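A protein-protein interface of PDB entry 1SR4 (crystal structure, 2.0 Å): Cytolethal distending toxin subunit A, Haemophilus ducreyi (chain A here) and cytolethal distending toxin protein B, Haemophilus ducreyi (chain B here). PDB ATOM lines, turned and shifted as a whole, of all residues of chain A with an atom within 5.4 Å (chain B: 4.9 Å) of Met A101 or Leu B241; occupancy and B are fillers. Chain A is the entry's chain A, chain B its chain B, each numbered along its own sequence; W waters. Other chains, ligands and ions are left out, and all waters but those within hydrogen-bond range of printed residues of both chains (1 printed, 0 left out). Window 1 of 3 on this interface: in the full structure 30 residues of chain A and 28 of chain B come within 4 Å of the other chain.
Met A101 touches three residues of chain B.
Leu B241 touches just these residues of chain A: Met A101 (3.7 Å), Leu A144 (3.6 Å) and Leu A195 (3.6 Å).
Of the printed residues of chain A, Asn B242 touches Met A101 (3.4 Å) and Phe A110 (3.6 Å).
Of the printed residues of chain B, Pro A103 touches Gln B35 (3.1 Å).
Printed residues of chain B within 4 Å of Leu A195: Leu B241 (3.6 Å) and Leu B244 (3.6 Å).
Printed residues of chain B within 4 Å of Glu A102: Gln B35 (3.5 Å).
Of the printed residues of chain A, Phe B253 touches Pro A146.
The nearest printed residue of chain B that does not touch Met A101 is Gln B243 (5.7 Å).
The nearest residue of chain A that does not touch Leu B241 is Phe A110 (4.2 Å).
The nearest printed residue of chain B that does not touch Pro A146 is Leu B241 (5.3 Å).
Of the 16 printed residues of chain A, 7 touch a printed residue of chain B.
Printed residues of chain A that touch a printed residue of chain B: Met A101, Glu A102, Pro A103, Phe A110, Leu A144, Pro A146 and Leu A195.
Printed residues of chain B that touch a printed residue of chain A: Gln B35, Leu B239, Leu B241, Asn B242, Leu B244 and Phe B253.
Hydrophobic or aromatic side chains of chain B that line the printed part of chain A: Leu B239, Leu B241 and Phe B253.
Among the printed residues, no Asp or Glu carboxylate lies within 4 Å of a Lys or Arg side-chain nitrogen of the other chain.
Water W1 lies within hydrogen-bond range of OD1 of Asn A59 (2.7 Å) and N of Gln B35 (3.1 Å).
Among the printed residues, pairs that only touch across the chains: Pro A103 with Gln B35 (3.1 Å), Phe A110 with Leu B239 (3.4 Å), Met A101 with Asn B242 (3.4 Å), Glu A102 with Gln B35 (3.5 Å), Pro A146 with Phe B253 (3.5 Å), Phe A110 with Asn B242 (3.6 Å), Leu A144 with Leu B241 (3.6 Å), Leu A195 with Leu B241 (3.6 Å), Leu A195 with Leu B244 (3.6 Å), Met A101 with Leu B241 (3.7 Å) and Pro A146 with Leu B239 (3.8 Å).
O of Met A101 sits at hydrogen-bond distance from NE2 of Gln B35.
OE1 of Glu A102 is in salt-bridge range of NH2 of Arg A111.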
ATOM      1  N   ASN A  59     -14.039 -11.895  17.929  1.00  0.00           N
ATOM      2  CA  ASN A  59     -13.129 -13.017  18.112  1.00  0.00           C
ATOM      3  C   ASN A  59     -12.661 -13.710  16.839  1.00  0.00           C
ATOM      4  O   ASN A  59     -11.775 -14.568  16.889  1.00  0.00           O
ATOM      5  CB  ASN A  59     -13.761 -14.045  19.049  1.00  0.00           C
ATOM      6  CG  ASN A  59     -14.093 -13.453  20.405  1.00  0.00           C
ATOM      7  OD1 ASN A  59     -13.258 -12.794  21.020  1.00  0.00           O
ATOM      8  ND2 ASN A  59     -15.315 -13.678  20.876  1.00  0.00           N
ATOM      9  N   MET A  61     -11.588 -13.697  12.458  1.00  0.00           N
ATOM     10  CA  MET A  61     -10.886 -12.963  11.423  1.00  0.00           C
ATOM     11  C   MET A  61     -10.734 -13.854  10.203  1.00  0.00           C
ATOM     12  O   MET A  61     -11.198 -15.003  10.201  1.00  0.00           O
ATOM     13  CB  MET A  61      -9.508 -12.558  11.955  1.00  0.00           C
ATOM     14  CG  MET A  61      -8.731 -13.688  12.659  1.00  0.00           C
ATOM     15  SD  MET A  61      -7.952 -14.899  11.560  1.00  0.00           S
ATOM     16  CE  MET A  61      -6.470 -13.978  11.118  1.00  0.00           C
ATOM     17  N   TRP A  99     -12.019 -17.651  11.077  1.00  0.00           N
ATOM     18  CA  TRP A  99     -11.256 -18.387  12.061  1.00  0.00           C
ATOM     19  C   TRP A  99     -10.990 -17.550  13.295  1.00  0.00           C
ATOM     20  O   TRP A  99     -10.949 -16.316  13.232  1.00  0.00           O
ATOM     21  CB  TRP A  99      -9.898 -18.795  11.479  1.00  0.00           C
ATOM     22  CG  TRP A  99      -9.978 -19.516  10.164  1.00  0.00           C
ATOM     23  CD1 TRP A  99     -10.042 -18.955   8.919  1.00  0.00           C
ATOM     24  CD2 TRP A  99     -10.003 -20.933   9.972  1.00  0.00           C
ATOM     25  NE1 TRP A  99     -10.103 -19.943   7.958  1.00  0.00           N
ATOM     26  CE2 TRP A  99     -10.075 -21.166   8.579  1.00  0.00           C
ATOM     27  CE3 TRP A  99      -9.967 -22.032  10.847  1.00  0.00           C
ATOM     28  CZ2 TRP A  99     -10.109 -22.455   8.032  1.00  0.00           C
ATOM     29  CZ3 TRP A  99     -10.001 -23.321  10.302  1.00  0.00           C
ATOM     30  CH2 TRP A  99     -10.070 -23.516   8.904  1.00  0.00           C
ATOM     31  N   LYS A 100     -10.801 -18.245  14.410  1.00  0.00           N
ATOM     32  CA  LYS A 100     -10.454 -17.626  15.670  1.00  0.00           C
ATOM     33  C   LYS A 100      -8.974 -17.988  15.862  1.00  0.00           C
ATOM     34  O   LYS A 100      -8.596 -19.163  15.890  1.00  0.00           O
ATOM     35  CB  LYS A 100     -11.289 -18.199  16.817  1.00  0.00           C
ATOM     36  CG  LYS A 100     -10.806 -17.760  18.207  1.00  0.00           C
ATOM     37  CD  LYS A 100     -11.604 -18.428  19.342  1.00  0.00           C
ATOM     38  CE  LYS A 100     -13.035 -17.921  19.384  1.00  0.00           C
ATOM     39  NZ  LYS A 100     -13.872 -18.557  20.467  1.00  0.00           N
ATOM     40  N   MET A 101      -8.141 -16.969  15.970  1.00  0.00           N
ATOM     41  CA  MET A 101      -6.711 -17.148  16.157  1.00  0.00           C
ATOM     42  C   MET A 101      -6.381 -17.143  17.662  1.00  0.00           C
ATOM     43  O   MET A 101      -6.644 -16.157  18.348  1.00  0.00           O
ATOM     44  CB  MET A 101      -6.000 -15.994  15.465  1.00  0.00           C
ATOM     45  CG  MET A 101      -4.629 -16.292  15.001  1.00  0.00           C
ATOM     46  SD  MET A 101      -3.898 -14.872  14.138  1.00  0.00           S
ATOM     47  CE  MET A 101      -2.384 -15.040  14.832  1.00  0.00           C
ATOM     48  N   GLU A 102      -5.808 -18.237  18.161  1.00  0.00           N
ATOM     49  CA  GLU A 102      -5.440 -18.361  19.574  1.00  0.00           C
ATOM     50  C   GLU A 102      -3.994 -18.782  19.736  1.00  0.00           C
ATOM     51  O   GLU A 102      -3.405 -19.392  18.835  1.00  0.00           O
ATOM     52  CB  GLU A 102      -6.261 -19.441  20.280  1.00  0.00           C
ATOM     53  CG  GLU A 102      -7.723 -19.446  19.974  1.00  0.00           C
ATOM     54  CD  GLU A 102      -8.475 -20.520  20.747  1.00  0.00           C
ATOM     55  OE1 GLU A 102      -7.936 -21.630  20.938  1.00  0.00           O
ATOM     56  OE2 GLU A 102      -9.622 -20.253  21.153  1.00  0.00           O
ATOM     57  N   PRO A 103      -3.397 -18.463  20.898  1.00  0.00           N
ATOM     58  CA  PRO A 103      -2.015 -18.865  21.112  1.00  0.00           C
ATOM     59  C   PRO A 103      -2.030 -20.381  21.178  1.00  0.00           C
ATOM     60  O   PRO A 103      -3.026 -20.976  21.577  1.00  0.00           O
ATOM     61  CB  PRO A 103      -1.676 -18.223  22.459  1.00  0.00           C
ATOM     62  CG  PRO A 103      -2.438 -16.941  22.395  1.00  0.00           C
ATOM     63  CD  PRO A 103      -3.788 -17.422  21.871  1.00  0.00           C
ATOM     64  N   PHE A 110       0.621 -19.961  17.073  1.00  0.00           N
ATOM     65  CA  PHE A 110      -0.817 -19.771  17.026  1.00  0.00           C
ATOM     66  C   PHE A 110      -1.506 -20.932  16.336  1.00  0.00           C
ATOM     67  O   PHE A 110      -0.895 -21.673  15.550  1.00  0.00           O
ATOM     68  CB  PHE A 110      -1.142 -18.487  16.263  1.00  0.00           C
ATOM     69  CG  PHE A 110      -0.654 -17.249  16.948  1.00  0.00           C
ATOM     70  CD1 PHE A 110      -1.371 -16.701  18.007  1.00  0.00           C
ATOM     71  CD2 PHE A 110       0.548 -16.649  16.558  1.00  0.00           C
ATOM     72  CE1 PHE A 110      -0.909 -15.567  18.681  1.00  0.00           C
ATOM     73  CE2 PHE A 110       1.023 -15.514  17.225  1.00  0.00           C
ATOM     74  CZ  PHE A 110       0.285 -14.974  18.291  1.00  0.00           C
ATOM     75  N   ARG A 111      -2.781 -21.086  16.648  1.00  0.00           N
ATOM     76  CA  ARG A 111      -3.594 -22.109  16.028  1.00  0.00           C
ATOM     77  C   ARG A 111      -4.856 -21.390  15.567  1.00  0.00           C
ATOM     78  O   ARG A 111      -5.197 -20.318  16.093  1.00  0.00           O
ATOM     79  CB  ARG A 111      -3.927 -23.208  17.009  1.00  0.00           C
ATOM     80  CG  ARG A 111      -4.946 -22.827  18.031  1.00  0.00           C
ATOM     81  CD  ARG A 111      -5.483 -24.086  18.638  1.00  0.00           C
ATOM     82  NE  ARG A 111      -6.506 -23.842  19.641  1.00  0.00           N
ATOM     83  CZ  ARG A 111      -7.026 -24.802  20.394  1.00  0.00           C
ATOM     84  NH1 ARG A 111      -6.611 -26.053  20.237  1.00  0.00           N
ATOM     85  NH2 ARG A 111      -7.938 -24.506  21.311  1.00  0.00           N
ATOM     86  N   PHE A 112      -5.538 -21.971  14.585  1.00  0.00           N
ATOM     87  CA  PHE A 112      -6.742 -21.379  14.007  1.00  0.00           C
ATOM     88  C   PHE A 112      -7.949 -22.303  14.114  1.00  0.00           C
ATOM     89  O   PHE A 112      -7.951 -23.404  13.565  1.00  0.00           O
ATOM     90  CB  PHE A 112      -6.477 -21.038  12.541  1.00  0.00           C
ATOM     91  CG  PHE A 112      -5.368 -20.037  12.346  1.00  0.00           C
ATOM     92  CD1 PHE A 112      -5.648 -18.675  12.286  1.00  0.00           C
ATOM     93  CD2 PHE A 112      -4.041 -20.459  12.263  1.00  0.00           C
ATOM     94  CE1 PHE A 112      -4.621 -17.748  12.149  1.00  0.00           C
ATOM     95  CE2 PHE A 112      -2.999 -19.537  12.124  1.00  0.00           C
ATOM     96  CZ  PHE A 112      -3.290 -18.179  12.067  1.00  0.00           C
ATOM     97  N   VAL A 113      -8.977 -21.830  14.807  1.00  0.00           N
ATOM     98  CA  VAL A 113     -10.203 -22.593  15.028  1.00  0.00           C
ATOM     99  C   VAL A 113     -11.331 -22.078  14.127  1.00  0.00           C
ATOM    100  O   VAL A 113     -11.667 -20.897  14.153  1.00  0.00           O
ATOM    101  CB  VAL A 113     -10.620 -22.473  16.500  1.00  0.00           C
ATOM    102  CG1 VAL A 113     -11.753 -23.478  16.828  1.00  0.00           C
ATOM    103  CG2 VAL A 113      -9.389 -22.722  17.389  1.00  0.00           C
ATOM    104  N   LEU A 144       3.815 -17.049  12.846  1.00  0.00           N
ATOM    105  CA  LEU A 144       3.589 -16.032  11.824  1.00  0.00           C
ATOM    106  C   LEU A 144       4.775 -15.090  11.883  1.00  0.00           C
ATOM    107  O   LEU A 144       5.091 -14.535  12.935  1.00  0.00           O
ATOM    108  CB  LEU A 144       2.276 -15.279  12.068  1.00  0.00           C
ATOM    109  CG  LEU A 144       1.017 -15.978  11.534  1.00  0.00           C
ATOM    110  CD1 LEU A 144       0.886 -17.364  12.157  1.00  0.00           C
ATOM    111  CD2 LEU A 144      -0.211 -15.124  11.835  1.00  0.00           C
ATOM    112  N   LEU A 145       5.439 -14.939  10.746  1.00  0.00           N
ATOM    113  CA  LEU A 145       6.618 -14.105  10.623  1.00  0.00           C
ATOM    114  C   LEU A 145       6.239 -12.773   9.973  1.00  0.00           C
ATOM    115  O   LEU A 145       5.815 -12.728   8.822  1.00  0.00           O
ATOM    116  CB  LEU A 145       7.654 -14.828   9.758  1.00  0.00           C
ATOM    117  CG  LEU A 145       7.842 -16.348   9.951  1.00  0.00           C
ATOM    118  CD1 LEU A 145       8.693 -16.908   8.810  1.00  0.00           C
ATOM    119  CD2 LEU A 145       8.492 -16.637  11.287  1.00  0.00           C
ATOM    120  N   PRO A 146       6.396 -11.671  10.699  1.00  0.00           N
ATOM    121  CA  PRO A 146       6.045 -10.371  10.115  1.00  0.00           C
ATOM    122  C   PRO A 146       6.981  -9.983   8.980  1.00  0.00           C
ATOM    123  O   PRO A 146       8.153 -10.361   8.985  1.00  0.00           O
ATOM    124  CB  PRO A 146       6.155  -9.416  11.310  1.00  0.00           C
ATOM    125  CG  PRO A 146       7.304 -10.016  12.104  1.00  0.00           C
ATOM    126  CD  PRO A 146       6.998 -11.524  12.038  1.00  0.00           C
ATOM    127  N   VAL A 152       2.095 -10.878   6.897  1.00  0.00           N
ATOM    128  CA  VAL A 152       2.781 -11.971   7.583  1.00  0.00           C
ATOM    129  C   VAL A 152       2.961 -13.189   6.678  1.00  0.00           C
ATOM    130  O   VAL A 152       2.248 -13.364   5.687  1.00  0.00           O
ATOM    131  CB  VAL A 152       2.010 -12.471   8.850  1.00  0.00           C
ATOM    132  CG1 VAL A 152       1.894 -11.368   9.896  1.00  0.00           C
ATOM    133  CG2 VAL A 152       0.612 -12.991   8.454  1.00  0.00           C
ATOM    134  N   LEU A 195      -3.781 -10.259   8.032  1.00  0.00           N
ATOM    135  CA  LEU A 195      -4.638 -10.610   9.158  1.00  0.00           C
ATOM    136  C   LEU A 195      -5.782  -9.623   8.933  1.00  0.00           C
ATOM    137  O   LEU A 195      -5.622  -8.423   9.153  1.00  0.00           O
ATOM    138  CB  LEU A 195      -3.877 -10.350  10.470  1.00  0.00           C
ATOM    139  CG  LEU A 195      -2.613 -11.244  10.540  1.00  0.00           C
ATOM    140  CD1 LEU A 195      -1.706 -10.869  11.689  1.00  0.00           C
ATOM    141  CD2 LEU A 195      -3.061 -12.685  10.654  1.00  0.00           C
ATOM    142  N   GLN B  35      -9.643 -12.231  23.910  1.00  0.00           N
ATOM    143  CA  GLN B  35      -8.196 -12.231  24.131  1.00  0.00           C
ATOM    144  C   GLN B  35      -7.573 -10.831  24.194  1.00  0.00           C
ATOM    145  O   GLN B  35      -6.356 -10.679  24.164  1.00  0.00           O
ATOM    146  CB  GLN B  35      -7.516 -13.069  23.042  1.00  0.00           C
ATOM    147  CG  GLN B  35      -8.085 -14.507  22.948  1.00  0.00           C
ATOM    148  CD  GLN B  35      -7.527 -15.321  21.774  1.00  0.00           C
ATOM    149  OE1 GLN B  35      -6.484 -15.959  21.884  1.00  0.00           O
ATOM    150  NE2 GLN B  35      -8.225 -15.291  20.646  1.00  0.00           N
ATOM    151  N   LEU B 239       4.354 -11.801  19.649  1.00  0.00           N
ATOM    152  CA  LEU B 239       3.820 -10.664  18.895  1.00  0.00           C
ATOM    153  C   LEU B 239       2.312 -10.898  19.049  1.00  0.00           C
ATOM    154  O   LEU B 239       1.853 -12.039  18.948  1.00  0.00           O
ATOM    155  CB  LEU B 239       4.226 -10.736  17.414  1.00  0.00           C
ATOM    156  CG  LEU B 239       5.738 -10.669  17.139  1.00  0.00           C
ATOM    157  CD1 LEU B 239       6.009 -10.656  15.642  1.00  0.00           C
ATOM    158  CD2 LEU B 239       6.311  -9.403  17.800  1.00  0.00           C
ATOM    159  N   MET B 240       1.540  -9.846  19.312  1.00  0.00           N
ATOM    160  CA  MET B 240       0.090 -10.002  19.511  1.00  0.00           C
ATOM    161  C   MET B 240      -0.686 -10.010  18.191  1.00  0.00           C
ATOM    162  O   MET B 240      -1.645  -9.257  18.006  1.00  0.00           O
ATOM    163  CB  MET B 240      -0.441  -8.877  20.414  1.00  0.00           C
ATOM    164  CG  MET B 240      -1.863  -9.125  20.928  1.00  0.00           C
ATOM    165  SD  MET B 240      -2.241  -7.924  22.192  1.00  0.00           S
ATOM    166  CE  MET B 240      -3.372  -8.830  23.236  1.00  0.00           C
ATOM    167  N   LEU B 241      -0.293 -10.902  17.295  1.00  0.00           N
ATOM    168  CA  LEU B 241      -0.903 -10.963  15.980  1.00  0.00           C
ATOM    169  C   LEU B 241      -2.323 -11.479  15.963  1.00  0.00           C
ATOM    170  O   LEU B 241      -3.056 -11.230  15.012  1.00  0.00           O
ATOM    171  CB  LEU B 241      -0.021 -11.791  15.048  1.00  0.00           C
ATOM    172  CG  LEU B 241       1.445 -11.347  14.969  1.00  0.00           C
ATOM    173  CD1 LEU B 241       2.218 -12.331  14.102  1.00  0.00           C
ATOM    174  CD2 LEU B 241       1.545  -9.933  14.407  1.00  0.00           C
ATOM    175  N   ASN B 242      -2.725 -12.190  17.012  1.00  0.00           N
ATOM    176  CA  ASN B 242      -4.084 -12.720  17.075  1.00  0.00           C
ATOM    177  C   ASN B 242      -5.142 -11.614  17.226  1.00  0.00           C
ATOM    178  O   ASN B 242      -6.336 -11.856  17.043  1.00  0.00           O
ATOM    179  CB  ASN B 242      -4.193 -13.734  18.221  1.00  0.00           C
ATOM    180  CG  ASN B 242      -3.763 -13.168  19.548  1.00  0.00           C
ATOM    181  OD1 ASN B 242      -2.670 -12.618  19.683  1.00  0.00           O
ATOM    182  ND2 ASN B 242      -4.621 -13.307  20.545  1.00  0.00           N
ATOM    183  N   GLN B 243      -4.695 -10.398  17.529  1.00  0.00           N
ATOM    184  CA  GLN B 243      -5.618  -9.282  17.703  1.00  0.00           C
ATOM    185  C   GLN B 243      -5.814  -8.399  16.456  1.00  0.00           C
ATOM    186  O   GLN B 243      -6.812  -7.672  16.362  1.00  0.00           O
ATOM    187  CB  GLN B 243      -5.149  -8.400  18.858  1.00  0.00           C
ATOM    188  CG  GLN B 243      -5.291  -9.017  20.246  1.00  0.00           C
ATOM    189  CD  GLN B 243      -6.716  -9.456  20.567  1.00  0.00           C
ATOM    190  OE1 GLN B 243      -7.045 -10.634  20.463  1.00  0.00           O
ATOM    191  NE2 GLN B 243      -7.566  -8.505  20.956  1.00  0.00           N
ATOM    192  N   LEU B 244      -4.904  -8.505  15.488  1.00  0.00           N
ATOM    193  CA  LEU B 244      -4.952  -7.664  14.290  1.00  0.00           C
ATOM    194  C   LEU B 244      -6.000  -8.005  13.222  1.00  0.00           C
ATOM    195  O   LEU B 244      -6.244  -9.171  12.921  1.00  0.00           O
ATOM    196  CB  LEU B 244      -3.557  -7.624  13.646  1.00  0.00           C
ATOM    197  CG  LEU B 244      -2.400  -7.389  14.628  1.00  0.00           C
ATOM    198  CD1 LEU B 244      -1.091  -7.285  13.864  1.00  0.00           C
ATOM    199  CD2 LEU B 244      -2.633  -6.111  15.421  1.00  0.00           C
ATOM    200  N   ILE B 248      -0.691  -2.576  10.752  1.00  0.00           N
ATOM    201  CA  ILE B 248      -0.198  -2.048  12.025  1.00  0.00           C
ATOM    202  C   ILE B 248       0.341  -0.693  11.603  1.00  0.00           C
ATOM    203  O   ILE B 248       1.244  -0.623  10.768  1.00  0.00           O
ATOM    204  CB  ILE B 248       0.939  -2.914  12.615  1.00  0.00           C
ATOM    205  CG1 ILE B 248       0.405  -4.312  12.929  1.00  0.00           C
ATOM    206  CG2 ILE B 248       1.467  -2.285  13.922  1.00  0.00           C
ATOM    207  CD1 ILE B 248       1.398  -5.187  13.667  1.00  0.00           C
ATOM    208  N   PHE B 253       5.637  -3.751  16.279  1.00  0.00           N
ATOM    209  CA  PHE B 253       4.564  -4.736  16.340  1.00  0.00           C
ATOM    210  C   PHE B 253       4.148  -4.853  17.809  1.00  0.00           C
ATOM    211  O   PHE B 253       4.996  -4.853  18.702  1.00  0.00           O
ATOM    212  CB  PHE B 253       5.078  -6.079  15.811  1.00  0.00           C
ATOM    213  CG  PHE B 253       5.365  -6.067  14.330  1.00  0.00           C
ATOM    214  CD1 PHE B 253       4.371  -6.405  13.417  1.00  0.00           C
ATOM    215  CD2 PHE B 253       6.598  -5.656  13.853  1.00  0.00           C
ATOM    216  CE1 PHE B 253       4.600  -6.328  12.050  1.00  0.00           C
ATOM    217  CE2 PHE B 253       6.842  -5.574  12.490  1.00  0.00           C
ATOM    218  CZ  PHE B 253       5.832  -5.914  11.583  1.00  0.00           C
HETATM  219  O   HOH W   1     -10.576 -12.623  20.936  1.00  0.00           O
